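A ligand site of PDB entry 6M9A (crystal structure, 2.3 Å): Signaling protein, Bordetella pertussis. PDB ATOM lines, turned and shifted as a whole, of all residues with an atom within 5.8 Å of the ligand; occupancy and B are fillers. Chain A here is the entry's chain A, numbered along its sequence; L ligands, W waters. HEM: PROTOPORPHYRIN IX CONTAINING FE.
Residues that only touch the ligand: Phe 52 (3.8 Å), Met 56 (3.7 Å), Ala 62 (3.4 Å), Phe 65 (3.7 Å), Leu 66 (3.6 Å), Leu 70 (3.9 Å), Leu 75 (3.7 Å), Ser 78 (3.96 Å), Met 79 (3.7 Å), Trp 82 (3.3 Å), Val 105 (3.8 Å), Val 108 (3.9 Å), Ile 112 (3.5 Å), Ile 114 (3.7 Å), Leu 118 (3.6 Å), Val 119 (3.7 Å), Gly 122 (3.9 Å) and Ala 123 (3.5 Å).
Hydrophobic or aromatic side chains within 4 Å of the ligand: Phe 52, Met 56, Ala 62, Phe 65, Leu 66, Leu 70, Leu 75, Met 79, Trp 82, Val 105, Val 108, His 109, Ile 112, Ile 114, Leu 118 and Val 119.
Within 4 Å of the ligand: Phe 52, Met 56, Ala 62, Phe 65, Leu 66, Leu 70, Lys 74, Leu 75, Ser 78, Met 79, Trp 82, Val 105, Val 108, His 109, Ile 112, Ile 114, Leu 118, Val 119, Gly 122 and Ala 123.
Along chain A the residues within 4 Å of the ligand span positions 52 to 123.
The nearest printed residue that does not touch the ligand is Met 163 (4.03 Å).
Water W1 lies within hydrogen-bond range of OH of Tyr 53 (2.9 Å), N of Met 79 (3.0 Å) and O of Leu 75 (3.1 Å).
The backbone carbonyl oxygen (O) of His 109 sits at hydrogen-bond distance from the backbone NH (N) of Ile 114 (2.9 Å).
A ring nitrogen (ND1) of His 109 lies within hydrogen-bond range of the backbone carbonyl oxygen (O) of Val 105 (3.0 Å).
The side-chain hydroxyl (OG) of Ser 78 is in hydrogen-bond range of the backbone carbonyl oxygen (O) of Lys 74, at 2.6 Å.
N of Leu 75 sits at hydrogen-bond distance from O of Leu 70 (2.9 Å).
An iron atom (FE) of the ligand is bound by a ring nitrogen (NE2) of His 109.
O2D of the ligand lies within salt-bridge range of NZ of Lys 74 (2.5 Å).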
ATOM      1  N   PHE A  52     -12.235  -2.752  14.784  1.00  0.00           N
ATOM      2  CA  PHE A  52     -12.761  -4.022  14.263  1.00  0.00           C
ATOM      3  C   PHE A  52     -13.047  -4.998  15.402  1.00  0.00           C
ATOM      4  O   PHE A  52     -14.154  -5.548  15.505  1.00  0.00           O
ATOM      5  CB  PHE A  52     -11.799  -4.618  13.222  1.00  0.00           C
ATOM      6  CG  PHE A  52     -12.257  -5.929  12.604  1.00  0.00           C
ATOM      7  CD1 PHE A  52     -12.776  -5.959  11.313  1.00  0.00           C
ATOM      8  CD2 PHE A  52     -12.140  -7.143  13.295  1.00  0.00           C
ATOM      9  CE1 PHE A  52     -13.218  -7.166  10.733  1.00  0.00           C
ATOM     10  CE2 PHE A  52     -12.560  -8.342  12.723  1.00  0.00           C
ATOM     11  CZ  PHE A  52     -13.107  -8.357  11.442  1.00  0.00           C
ATOM     12  N   TYR A  53     -12.072  -5.208  16.292  1.00  0.00           N
ATOM     13  CA  TYR A  53     -12.239  -6.236  17.303  1.00  0.00           C
ATOM     14  C   TYR A  53     -13.097  -5.800  18.479  1.00  0.00           C
ATOM     15  O   TYR A  53     -13.669  -6.650  19.153  1.00  0.00           O
ATOM     16  CB  TYR A  53     -10.856  -6.753  17.770  1.00  0.00           C
ATOM     17  CG  TYR A  53     -10.296  -7.626  16.677  1.00  0.00           C
ATOM     18  CD1 TYR A  53     -10.852  -8.880  16.431  1.00  0.00           C
ATOM     19  CD2 TYR A  53      -9.293  -7.179  15.836  1.00  0.00           C
ATOM     20  CE1 TYR A  53     -10.388  -9.683  15.394  1.00  0.00           C
ATOM     21  CE2 TYR A  53      -8.814  -7.985  14.787  1.00  0.00           C
ATOM     22  CZ  TYR A  53      -9.373  -9.234  14.582  1.00  0.00           C
ATOM     23  OH  TYR A  53      -8.937 -10.022  13.556  1.00  0.00           O
ATOM     24  N   MET A  56     -16.568  -6.781  17.129  1.00  0.00           N
ATOM     25  CA  MET A  56     -16.765  -8.223  17.169  1.00  0.00           C
ATOM     26  C   MET A  56     -16.879  -8.751  18.606  1.00  0.00           C
ATOM     27  O   MET A  56     -17.744  -9.576  18.898  1.00  0.00           O
ATOM     28  CB  MET A  56     -15.614  -8.920  16.440  1.00  0.00           C
ATOM     29  CG  MET A  56     -15.627  -8.730  14.915  1.00  0.00           C
ATOM     30  SD  MET A  56     -17.161  -9.331  14.186  1.00  0.00           S
ATOM     31  CE  MET A  56     -17.019  -8.657  12.553  1.00  0.00           C
ATOM     32  N   ALA A  62     -20.605 -13.215  17.757  1.00  0.00           N
ATOM     33  CA  ALA A  62     -19.247 -13.206  17.218  1.00  0.00           C
ATOM     34  C   ALA A  62     -18.203 -13.462  18.313  1.00  0.00           C
ATOM     35  O   ALA A  62     -17.169 -14.090  18.039  1.00  0.00           O
ATOM     36  CB  ALA A  62     -18.971 -11.871  16.534  1.00  0.00           C
ATOM     37  N   ALA A  63     -18.477 -13.019  19.530  1.00  0.00           N
ATOM     38  CA  ALA A  63     -17.550 -13.239  20.633  1.00  0.00           C
ATOM     39  C   ALA A  63     -17.438 -14.723  20.922  1.00  0.00           C
ATOM     40  O   ALA A  63     -16.577 -15.136  21.687  1.00  0.00           O
ATOM     41  CB  ALA A  63     -18.002 -12.485  21.870  1.00  0.00           C
ATOM     42  N   PHE A  65     -16.573 -17.036  18.812  1.00  0.00           N
ATOM     43  CA  PHE A  65     -15.396 -17.523  18.087  1.00  0.00           C
ATOM     44  C   PHE A  65     -14.093 -16.854  18.526  1.00  0.00           C
ATOM     45  O   PHE A  65     -13.021 -17.220  18.021  1.00  0.00           O
ATOM     46  CB  PHE A  65     -15.610 -17.313  16.587  1.00  0.00           C
ATOM     47  CG  PHE A  65     -16.886 -17.933  16.073  1.00  0.00           C
ATOM     48  CD1 PHE A  65     -16.921 -19.255  15.673  1.00  0.00           C
ATOM     49  CD2 PHE A  65     -18.064 -17.202  16.023  1.00  0.00           C
ATOM     50  CE1 PHE A  65     -18.098 -19.841  15.218  1.00  0.00           C
ATOM     51  CE2 PHE A  65     -19.240 -17.776  15.582  1.00  0.00           C
ATOM     52  CZ  PHE A  65     -19.261 -19.089  15.182  1.00  0.00           C
ATOM     53  N   LEU A  66     -14.132 -15.879  19.436  1.00  0.00           N
ATOM     54  CA  LEU A  66     -12.947 -15.122  19.805  1.00  0.00           C
ATOM     55  C   LEU A  66     -12.672 -15.238  21.305  1.00  0.00           C
ATOM     56  O   LEU A  66     -13.570 -15.081  22.134  1.00  0.00           O
ATOM     57  CB  LEU A  66     -13.103 -13.653  19.422  1.00  0.00           C
ATOM     58  CG  LEU A  66     -13.368 -13.456  17.927  1.00  0.00           C
ATOM     59  CD1 LEU A  66     -13.788 -12.020  17.651  1.00  0.00           C
ATOM     60  CD2 LEU A  66     -12.125 -13.847  17.145  1.00  0.00           C
ATOM     61  N   LEU A  70      -6.604 -14.501  21.903  1.00  0.00           N
ATOM     62  CA  LEU A  70      -6.359 -14.640  20.473  1.00  0.00           C
ATOM     63  C   LEU A  70      -6.274 -13.276  19.807  1.00  0.00           C
ATOM     64  O   LEU A  70      -5.396 -13.025  18.967  1.00  0.00           O
ATOM     65  CB  LEU A  70      -7.469 -15.497  19.858  1.00  0.00           C
ATOM     66  CG  LEU A  70      -7.391 -15.912  18.387  1.00  0.00           C
ATOM     67  CD1 LEU A  70      -6.126 -16.719  18.152  1.00  0.00           C
ATOM     68  CD2 LEU A  70      -8.644 -16.712  18.011  1.00  0.00           C
ATOM     69  N   LYS A  74      -2.590 -12.336  18.533  1.00  0.00           N
ATOM     70  CA  LYS A  74      -2.496 -12.793  17.155  1.00  0.00           C
ATOM     71  C   LYS A  74      -3.305 -11.934  16.187  1.00  0.00           C
ATOM     72  O   LYS A  74      -2.736 -11.346  15.268  1.00  0.00           O
ATOM     73  CB  LYS A  74      -2.911 -14.253  17.052  1.00  0.00           C
ATOM     74  CG  LYS A  74      -2.802 -14.826  15.660  1.00  0.00           C
ATOM     75  CD  LYS A  74      -3.124 -16.303  15.688  1.00  0.00           C
ATOM     76  CE  LYS A  74      -2.903 -16.928  14.332  1.00  0.00           C
ATOM     77  NZ  LYS A  74      -2.659 -18.400  14.443  1.00  0.00           N
ATOM     78  N   LEU A  75      -4.626 -11.813  16.404  1.00  0.00           N
ATOM     79  CA  LEU A  75      -5.480 -11.250  15.370  1.00  0.00           C
ATOM     80  C   LEU A  75      -5.346  -9.737  15.253  1.00  0.00           C
ATOM     81  O   LEU A  75      -5.496  -9.197  14.145  1.00  0.00           O
ATOM     82  CB  LEU A  75      -6.951 -11.584  15.599  1.00  0.00           C
ATOM     83  CG  LEU A  75      -7.265 -13.064  15.699  1.00  0.00           C
ATOM     84  CD1 LEU A  75      -8.748 -13.252  15.951  1.00  0.00           C
ATOM     85  CD2 LEU A  75      -6.793 -13.744  14.419  1.00  0.00           C
ATOM     86  N   SER A  78      -2.574  -9.542  12.893  1.00  0.00           N
ATOM     87  CA  SER A  78      -2.888 -10.120  11.586  1.00  0.00           C
ATOM     88  C   SER A  78      -3.857  -9.247  10.819  1.00  0.00           C
ATOM     89  O   SER A  78      -3.796  -9.175   9.585  1.00  0.00           O
ATOM     90  CB  SER A  78      -3.491 -11.512  11.761  1.00  0.00           C
ATOM     91  OG  SER A  78      -2.827 -12.221  12.799  1.00  0.00           O
ATOM     92  N   MET A  79      -4.773  -8.585  11.519  1.00  0.00           N
ATOM     93  CA  MET A  79      -5.687  -7.655  10.863  1.00  0.00           C
ATOM     94  C   MET A  79      -4.922  -6.453  10.288  1.00  0.00           C
ATOM     95  O   MET A  79      -5.211  -5.995   9.180  1.00  0.00           O
ATOM     96  CB  MET A  79      -6.759  -7.183  11.840  1.00  0.00           C
ATOM     97  CG  MET A  79      -7.645  -6.060  11.305  1.00  0.00           C
ATOM     98  SD  MET A  79      -8.609  -6.557   9.855  1.00  0.00           S
ATOM     99  CE  MET A  79      -9.658  -7.802  10.593  1.00  0.00           C
ATOM    100  N   TRP A  82      -3.304  -7.599   7.206  1.00  0.00           N
ATOM    101  CA  TRP A  82      -4.297  -7.861   6.174  1.00  0.00           C
ATOM    102  C   TRP A  82      -4.667  -6.563   5.461  1.00  0.00           C
ATOM    103  O   TRP A  82      -4.693  -6.501   4.223  1.00  0.00           O
ATOM    104  CB  TRP A  82      -5.522  -8.539   6.785  1.00  0.00           C
ATOM    105  CG  TRP A  82      -6.606  -8.875   5.791  1.00  0.00           C
ATOM    106  CD1 TRP A  82      -6.771 -10.048   5.120  1.00  0.00           C
ATOM    107  CD2 TRP A  82      -7.655  -8.013   5.356  1.00  0.00           C
ATOM    108  NE1 TRP A  82      -7.869  -9.965   4.308  1.00  0.00           N
ATOM    109  CE2 TRP A  82      -8.418  -8.720   4.418  1.00  0.00           C
ATOM    110  CE3 TRP A  82      -8.019  -6.689   5.662  1.00  0.00           C
ATOM    111  CZ2 TRP A  82      -9.547  -8.175   3.788  1.00  0.00           C
ATOM    112  CZ3 TRP A  82      -9.141  -6.143   5.040  1.00  0.00           C
ATOM    113  CH2 TRP A  82      -9.896  -6.890   4.122  1.00  0.00           C
ATOM    114  N   PHE A 101      -3.210 -14.927  -0.907  1.00  0.00           N
ATOM    115  CA  PHE A 101      -3.334 -14.673   0.524  1.00  0.00           C
ATOM    116  C   PHE A 101      -4.816 -14.556   0.945  1.00  0.00           C
ATOM    117  O   PHE A 101      -5.230 -15.166   1.942  1.00  0.00           O
ATOM    118  CB  PHE A 101      -2.550 -13.418   0.865  1.00  0.00           C
ATOM    119  CG  PHE A 101      -2.767 -12.901   2.256  1.00  0.00           C
ATOM    120  CD1 PHE A 101      -2.246 -13.575   3.351  1.00  0.00           C
ATOM    121  CD2 PHE A 101      -3.485 -11.734   2.471  1.00  0.00           C
ATOM    122  CE1 PHE A 101      -2.435 -13.096   4.628  1.00  0.00           C
ATOM    123  CE2 PHE A 101      -3.674 -11.254   3.747  1.00  0.00           C
ATOM    124  CZ  PHE A 101      -3.154 -11.940   4.829  1.00  0.00           C
ATOM    125  N   VAL A 105      -6.772 -16.949   3.692  1.00  0.00           N
ATOM    126  CA  VAL A 105      -7.476 -16.336   4.828  1.00  0.00           C
ATOM    127  C   VAL A 105      -8.929 -16.799   4.845  1.00  0.00           C
ATOM    128  O   VAL A 105      -9.440 -17.238   5.886  1.00  0.00           O
ATOM    129  CB  VAL A 105      -7.358 -14.807   4.751  1.00  0.00           C
ATOM    130  CG1 VAL A 105      -8.413 -14.144   5.648  1.00  0.00           C
ATOM    131  CG2 VAL A 105      -5.925 -14.382   5.080  1.00  0.00           C
ATOM    132  N   VAL A 108      -9.338 -20.198   6.318  1.00  0.00           N
ATOM    133  CA  VAL A 108      -9.219 -20.339   7.766  1.00  0.00           C
ATOM    134  C   VAL A 108     -10.576 -20.128   8.448  1.00  0.00           C
ATOM    135  O   VAL A 108     -10.924 -20.801   9.416  1.00  0.00           O
ATOM    136  CB  VAL A 108      -8.153 -19.373   8.314  1.00  0.00           C
ATOM    137  CG1 VAL A 108      -8.257 -19.242   9.834  1.00  0.00           C
ATOM    138  CG2 VAL A 108      -6.761 -19.850   7.919  1.00  0.00           C
ATOM    139  N   HIS A 109     -11.374 -19.210   7.917  1.00  0.00           N
ATOM    140  CA  HIS A 109     -12.670 -18.916   8.507  1.00  0.00           C
ATOM    141  C   HIS A 109     -13.692 -19.993   8.198  1.00  0.00           C
ATOM    142  O   HIS A 109     -14.468 -20.386   9.070  1.00  0.00           O
ATOM    143  CB  HIS A 109     -13.129 -17.539   8.028  1.00  0.00           C
ATOM    144  CG  HIS A 109     -12.271 -16.426   8.543  1.00  0.00           C
ATOM    145  ND1 HIS A 109     -11.239 -15.887   7.821  1.00  0.00           N
ATOM    146  CD2 HIS A 109     -12.276 -15.788   9.741  1.00  0.00           C
ATOM    147  CE1 HIS A 109     -10.642 -14.950   8.532  1.00  0.00           C
ATOM    148  NE2 HIS A 109     -11.263 -14.852   9.703  1.00  0.00           N
ATOM    149  N   ILE A 112     -13.226 -23.251  10.409  1.00  0.00           N
ATOM    150  CA  ILE A 112     -13.782 -23.201  11.762  1.00  0.00           C
ATOM    151  C   ILE A 112     -15.214 -22.682  11.771  1.00  0.00           C
ATOM    152  O   ILE A 112     -15.776 -22.472  12.840  1.00  0.00           O
ATOM    153  CB  ILE A 112     -12.896 -22.367  12.700  1.00  0.00           C
ATOM    154  CG1 ILE A 112     -12.637 -20.988  12.109  1.00  0.00           C
ATOM    155  CG2 ILE A 112     -11.579 -23.081  12.972  1.00  0.00           C
ATOM    156  CD1 ILE A 112     -11.545 -20.221  12.806  1.00  0.00           C
ATOM    157  N   ILE A 114     -16.690 -19.763  10.802  1.00  0.00           N
ATOM    158  CA  ILE A 114     -17.071 -18.380  11.071  1.00  0.00           C
ATOM    159  C   ILE A 114     -18.264 -18.093  10.155  1.00  0.00           C
ATOM    160  O   ILE A 114     -18.148 -18.263   8.927  1.00  0.00           O
ATOM    161  CB  ILE A 114     -15.911 -17.398  10.817  1.00  0.00           C
ATOM    162  CG1 ILE A 114     -14.673 -17.771  11.654  1.00  0.00           C
ATOM    163  CG2 ILE A 114     -16.351 -15.993  11.121  1.00  0.00           C
ATOM    164  CD1 ILE A 114     -14.918 -17.915  13.098  1.00  0.00           C
ATOM    165  N   PRO A 115     -19.413 -17.694  10.685  1.00  0.00           N
ATOM    166  CA  PRO A 115     -20.553 -17.346   9.830  1.00  0.00           C
ATOM    167  C   PRO A 115     -20.151 -16.256   8.842  1.00  0.00           C
ATOM    168  O   PRO A 115     -19.531 -15.261   9.204  1.00  0.00           O
ATOM    169  CB  PRO A 115     -21.608 -16.845  10.819  1.00  0.00           C
ATOM    170  CG  PRO A 115     -21.226 -17.445  12.123  1.00  0.00           C
ATOM    171  CD  PRO A 115     -19.722 -17.496  12.117  1.00  0.00           C
ATOM    172  N   LEU A 118     -20.903 -12.538   9.460  1.00  0.00           N
ATOM    173  CA  LEU A 118     -20.004 -11.804  10.348  1.00  0.00           C
ATOM    174  C   LEU A 118     -18.791 -11.273   9.590  1.00  0.00           C
ATOM    175  O   LEU A 118     -18.338 -10.146   9.845  1.00  0.00           O
ATOM    176  CB  LEU A 118     -19.568 -12.713  11.502  1.00  0.00           C
ATOM    177  CG  LEU A 118     -20.699 -13.166  12.413  1.00  0.00           C
ATOM    178  CD1 LEU A 118     -20.150 -13.869  13.628  1.00  0.00           C
ATOM    179  CD2 LEU A 118     -21.567 -11.964  12.834  1.00  0.00           C
ATOM    180  N   VAL A 119     -18.249 -12.064   8.657  1.00  0.00           N
ATOM    181  CA  VAL A 119     -17.175 -11.578   7.795  1.00  0.00           C
ATOM    182  C   VAL A 119     -17.626 -10.373   6.981  1.00  0.00           C
ATOM    183  O   VAL A 119     -16.918  -9.365   6.862  1.00  0.00           O
ATOM    184  CB  VAL A 119     -16.680 -12.725   6.890  1.00  0.00           C
ATOM    185  CG1 VAL A 119     -15.651 -12.215   5.921  1.00  0.00           C
ATOM    186  CG2 VAL A 119     -16.111 -13.870   7.748  1.00  0.00           C
ATOM    187  N   THR A 120     -18.837 -10.450   6.409  1.00  0.00           N
ATOM    188  CA  THR A 120     -19.420  -9.306   5.708  1.00  0.00           C
ATOM    189  C   THR A 120     -19.507  -8.090   6.620  1.00  0.00           C
ATOM    190  O   THR A 120     -19.093  -6.980   6.252  1.00  0.00           O
ATOM    191  CB  THR A 120     -20.816  -9.675   5.203  1.00  0.00           C
ATOM    192  OG1 THR A 120     -20.688 -10.583   4.098  1.00  0.00           O
ATOM    193  CG2 THR A 120     -21.607  -8.447   4.797  1.00  0.00           C
ATOM    194  N   GLY A 122     -17.858  -7.371   9.285  1.00  0.00           N
ATOM    195  CA  GLY A 122     -16.552  -6.831   9.591  1.00  0.00           C
ATOM    196  C   GLY A 122     -15.971  -6.016   8.451  1.00  0.00           C
ATOM    197  O   GLY A 122     -15.392  -4.941   8.664  1.00  0.00           O
ATOM    198  N   ALA A 123     -16.110  -6.505   7.231  1.00  0.00           N
ATOM    199  CA  ALA A 123     -15.729  -5.707   6.064  1.00  0.00           C
ATOM    200  C   ALA A 123     -16.448  -4.362   6.056  1.00  0.00           C
ATOM    201  O   ALA A 123     -15.833  -3.313   5.832  1.00  0.00           O
ATOM    202  CB  ALA A 123     -16.042  -6.484   4.796  1.00  0.00           C
ATOM    203  N   LEU A 126     -14.849  -2.005   8.511  1.00  0.00           N
ATOM    204  CA  LEU A 126     -13.605  -1.438   8.015  1.00  0.00           C
ATOM    205  C   LEU A 126     -13.871  -0.345   6.979  1.00  0.00           C
ATOM    206  O   LEU A 126     -13.207   0.694   6.988  1.00  0.00           O
ATOM    207  CB  LEU A 126     -12.696  -2.543   7.428  1.00  0.00           C
ATOM    208  CG  LEU A 126     -12.128  -3.527   8.444  1.00  0.00           C
ATOM    209  CD1 LEU A 126     -11.384  -4.688   7.787  1.00  0.00           C
ATOM    210  CD2 LEU A 126     -11.225  -2.811   9.434  1.00  0.00           C
ATOM    211  N   VAL A 160     -12.922  -9.302   0.256  1.00  0.00           N
ATOM    212  CA  VAL A 160     -13.870 -10.159   0.960  1.00  0.00           C
ATOM    213  C   VAL A 160     -14.473 -11.193   0.018  1.00  0.00           C
ATOM    214  O   VAL A 160     -14.729 -12.342   0.409  1.00  0.00           O
ATOM    215  CB  VAL A 160     -14.942  -9.303   1.660  1.00  0.00           C
ATOM    216  CG1 VAL A 160     -15.987 -10.161   2.328  1.00  0.00           C
ATOM    217  CG2 VAL A 160     -14.260  -8.443   2.679  1.00  0.00           C
ATOM    218  N   MET A 163     -11.952 -13.890  -0.087  1.00  0.00           N
ATOM    219  CA  MET A 163     -12.132 -14.637   1.145  1.00  0.00           C
ATOM    220  C   MET A 163     -13.359 -15.526   1.075  1.00  0.00           C
ATOM    221  O   MET A 163     -13.358 -16.643   1.603  1.00  0.00           O
ATOM    222  CB  MET A 163     -12.234 -13.692   2.333  1.00  0.00           C
ATOM    223  CG  MET A 163     -10.933 -13.231   2.905  1.00  0.00           C
ATOM    224  SD  MET A 163     -11.239 -12.088   4.253  1.00  0.00           S
ATOM    225  CE  MET A 163     -11.527 -10.636   3.313  1.00  0.00           C
HETATM  226  CHA HEM L   1      -7.948 -15.589  11.467  1.00  0.00           C
HETATM  227  CHB HEM L   1      -8.721 -11.418   9.068  1.00  0.00           C
HETATM  228  CHC HEM L   1     -13.409 -11.867  10.092  1.00  0.00           C
HETATM  229  CHD HEM L   1     -12.152 -14.831  13.731  1.00  0.00           C
HETATM  230  C1A HEM L   1      -7.739 -14.494  10.643  1.00  0.00           C
HETATM  231  C2A HEM L   1      -6.566 -14.186   9.853  1.00  0.00           C
HETATM  232  C3A HEM L   1      -6.795 -13.044   9.192  1.00  0.00           C
HETATM  233  C4A HEM L   1      -8.110 -12.563   9.536  1.00  0.00           C
HETATM  234  CMA HEM L   1      -5.815 -12.342   8.238  1.00  0.00           C
HETATM  235  CAA HEM L   1      -5.278 -15.023   9.731  1.00  0.00           C
HETATM  236  CBA HEM L   1      -4.572 -15.309  11.048  1.00  0.00           C
HETATM  237  CGA HEM L   1      -3.380 -16.173  10.679  1.00  0.00           C
HETATM  238  O1A HEM L   1      -2.314 -16.047  11.334  1.00  0.00           O
HETATM  239  O2A HEM L   1      -3.488 -16.983   9.709  1.00  0.00           O
HETATM  240  C1B HEM L   1     -10.087 -11.231   9.009  1.00  0.00           C
HETATM  241  C2B HEM L   1     -10.828 -10.329   8.141  1.00  0.00           C
HETATM  242  C3B HEM L   1     -12.128 -10.468   8.407  1.00  0.00           C
HETATM  243  C4B HEM L   1     -12.251 -11.443   9.486  1.00  0.00           C
HETATM  244  CMB HEM L   1     -10.177  -9.413   7.072  1.00  0.00           C
HETATM  245  CAB HEM L   1     -13.348  -9.738   7.776  1.00  0.00           C
HETATM  246  CBB HEM L   1     -13.319  -8.540   7.198  1.00  0.00           C
HETATM  247  C1C HEM L   1     -13.484 -12.638  11.234  1.00  0.00           C
HETATM  248  C2C HEM L   1     -14.638 -12.799  12.085  1.00  0.00           C
HETATM  249  C3C HEM L   1     -14.295 -13.642  13.096  1.00  0.00           C
HETATM  250  C4C HEM L   1     -12.909 -14.012  12.915  1.00  0.00           C
HETATM  251  CMC HEM L   1     -15.978 -12.105  11.793  1.00  0.00           C
HETATM  252  CAC HEM L   1     -15.142 -14.128  14.303  1.00  0.00           C
HETATM  253  CBC HEM L   1     -16.221 -13.490  14.787  1.00  0.00           C
HETATM  254  C1D HEM L   1     -10.956 -15.408  13.383  1.00  0.00           C
HETATM  255  C2D HEM L   1     -10.368 -16.634  13.910  1.00  0.00           C
HETATM  256  C3D HEM L   1      -9.209 -16.842  13.291  1.00  0.00           C
HETATM  257  C4D HEM L   1      -9.013 -15.771  12.334  1.00  0.00           C
HETATM  258  CMD HEM L   1     -10.970 -17.531  15.016  1.00  0.00           C
HETATM  259  CAD HEM L   1      -8.273 -18.055  13.549  1.00  0.00           C
HETATM  260  CBD HEM L   1      -7.046 -17.667  14.368  1.00  0.00           C
HETATM  261  CGD HEM L   1      -6.242 -18.905  14.697  1.00  0.00           C
HETATM  262  O1D HEM L   1      -6.719 -19.799  15.447  1.00  0.00           O
HETATM  263  O2D HEM L   1      -5.104 -19.012  14.214  1.00  0.00           O
HETATM  264  NA  HEM L   1      -8.652 -13.473  10.419  1.00  0.00           N
HETATM  265  NB  HEM L   1     -10.996 -11.878   9.811  1.00  0.00           N
HETATM  266  NC  HEM L   1     -12.459 -13.393  11.769  1.00  0.00           N
HETATM  267  ND  HEM L   1     -10.097 -14.922  12.441  1.00  0.00           N
HETATM  268 FE   HEM L   1     -10.558 -13.446  11.070  1.00  0.00          FE
HETATM  269  O   HOH W   1      -6.750 -10.799  11.762  1.00  0.00           O
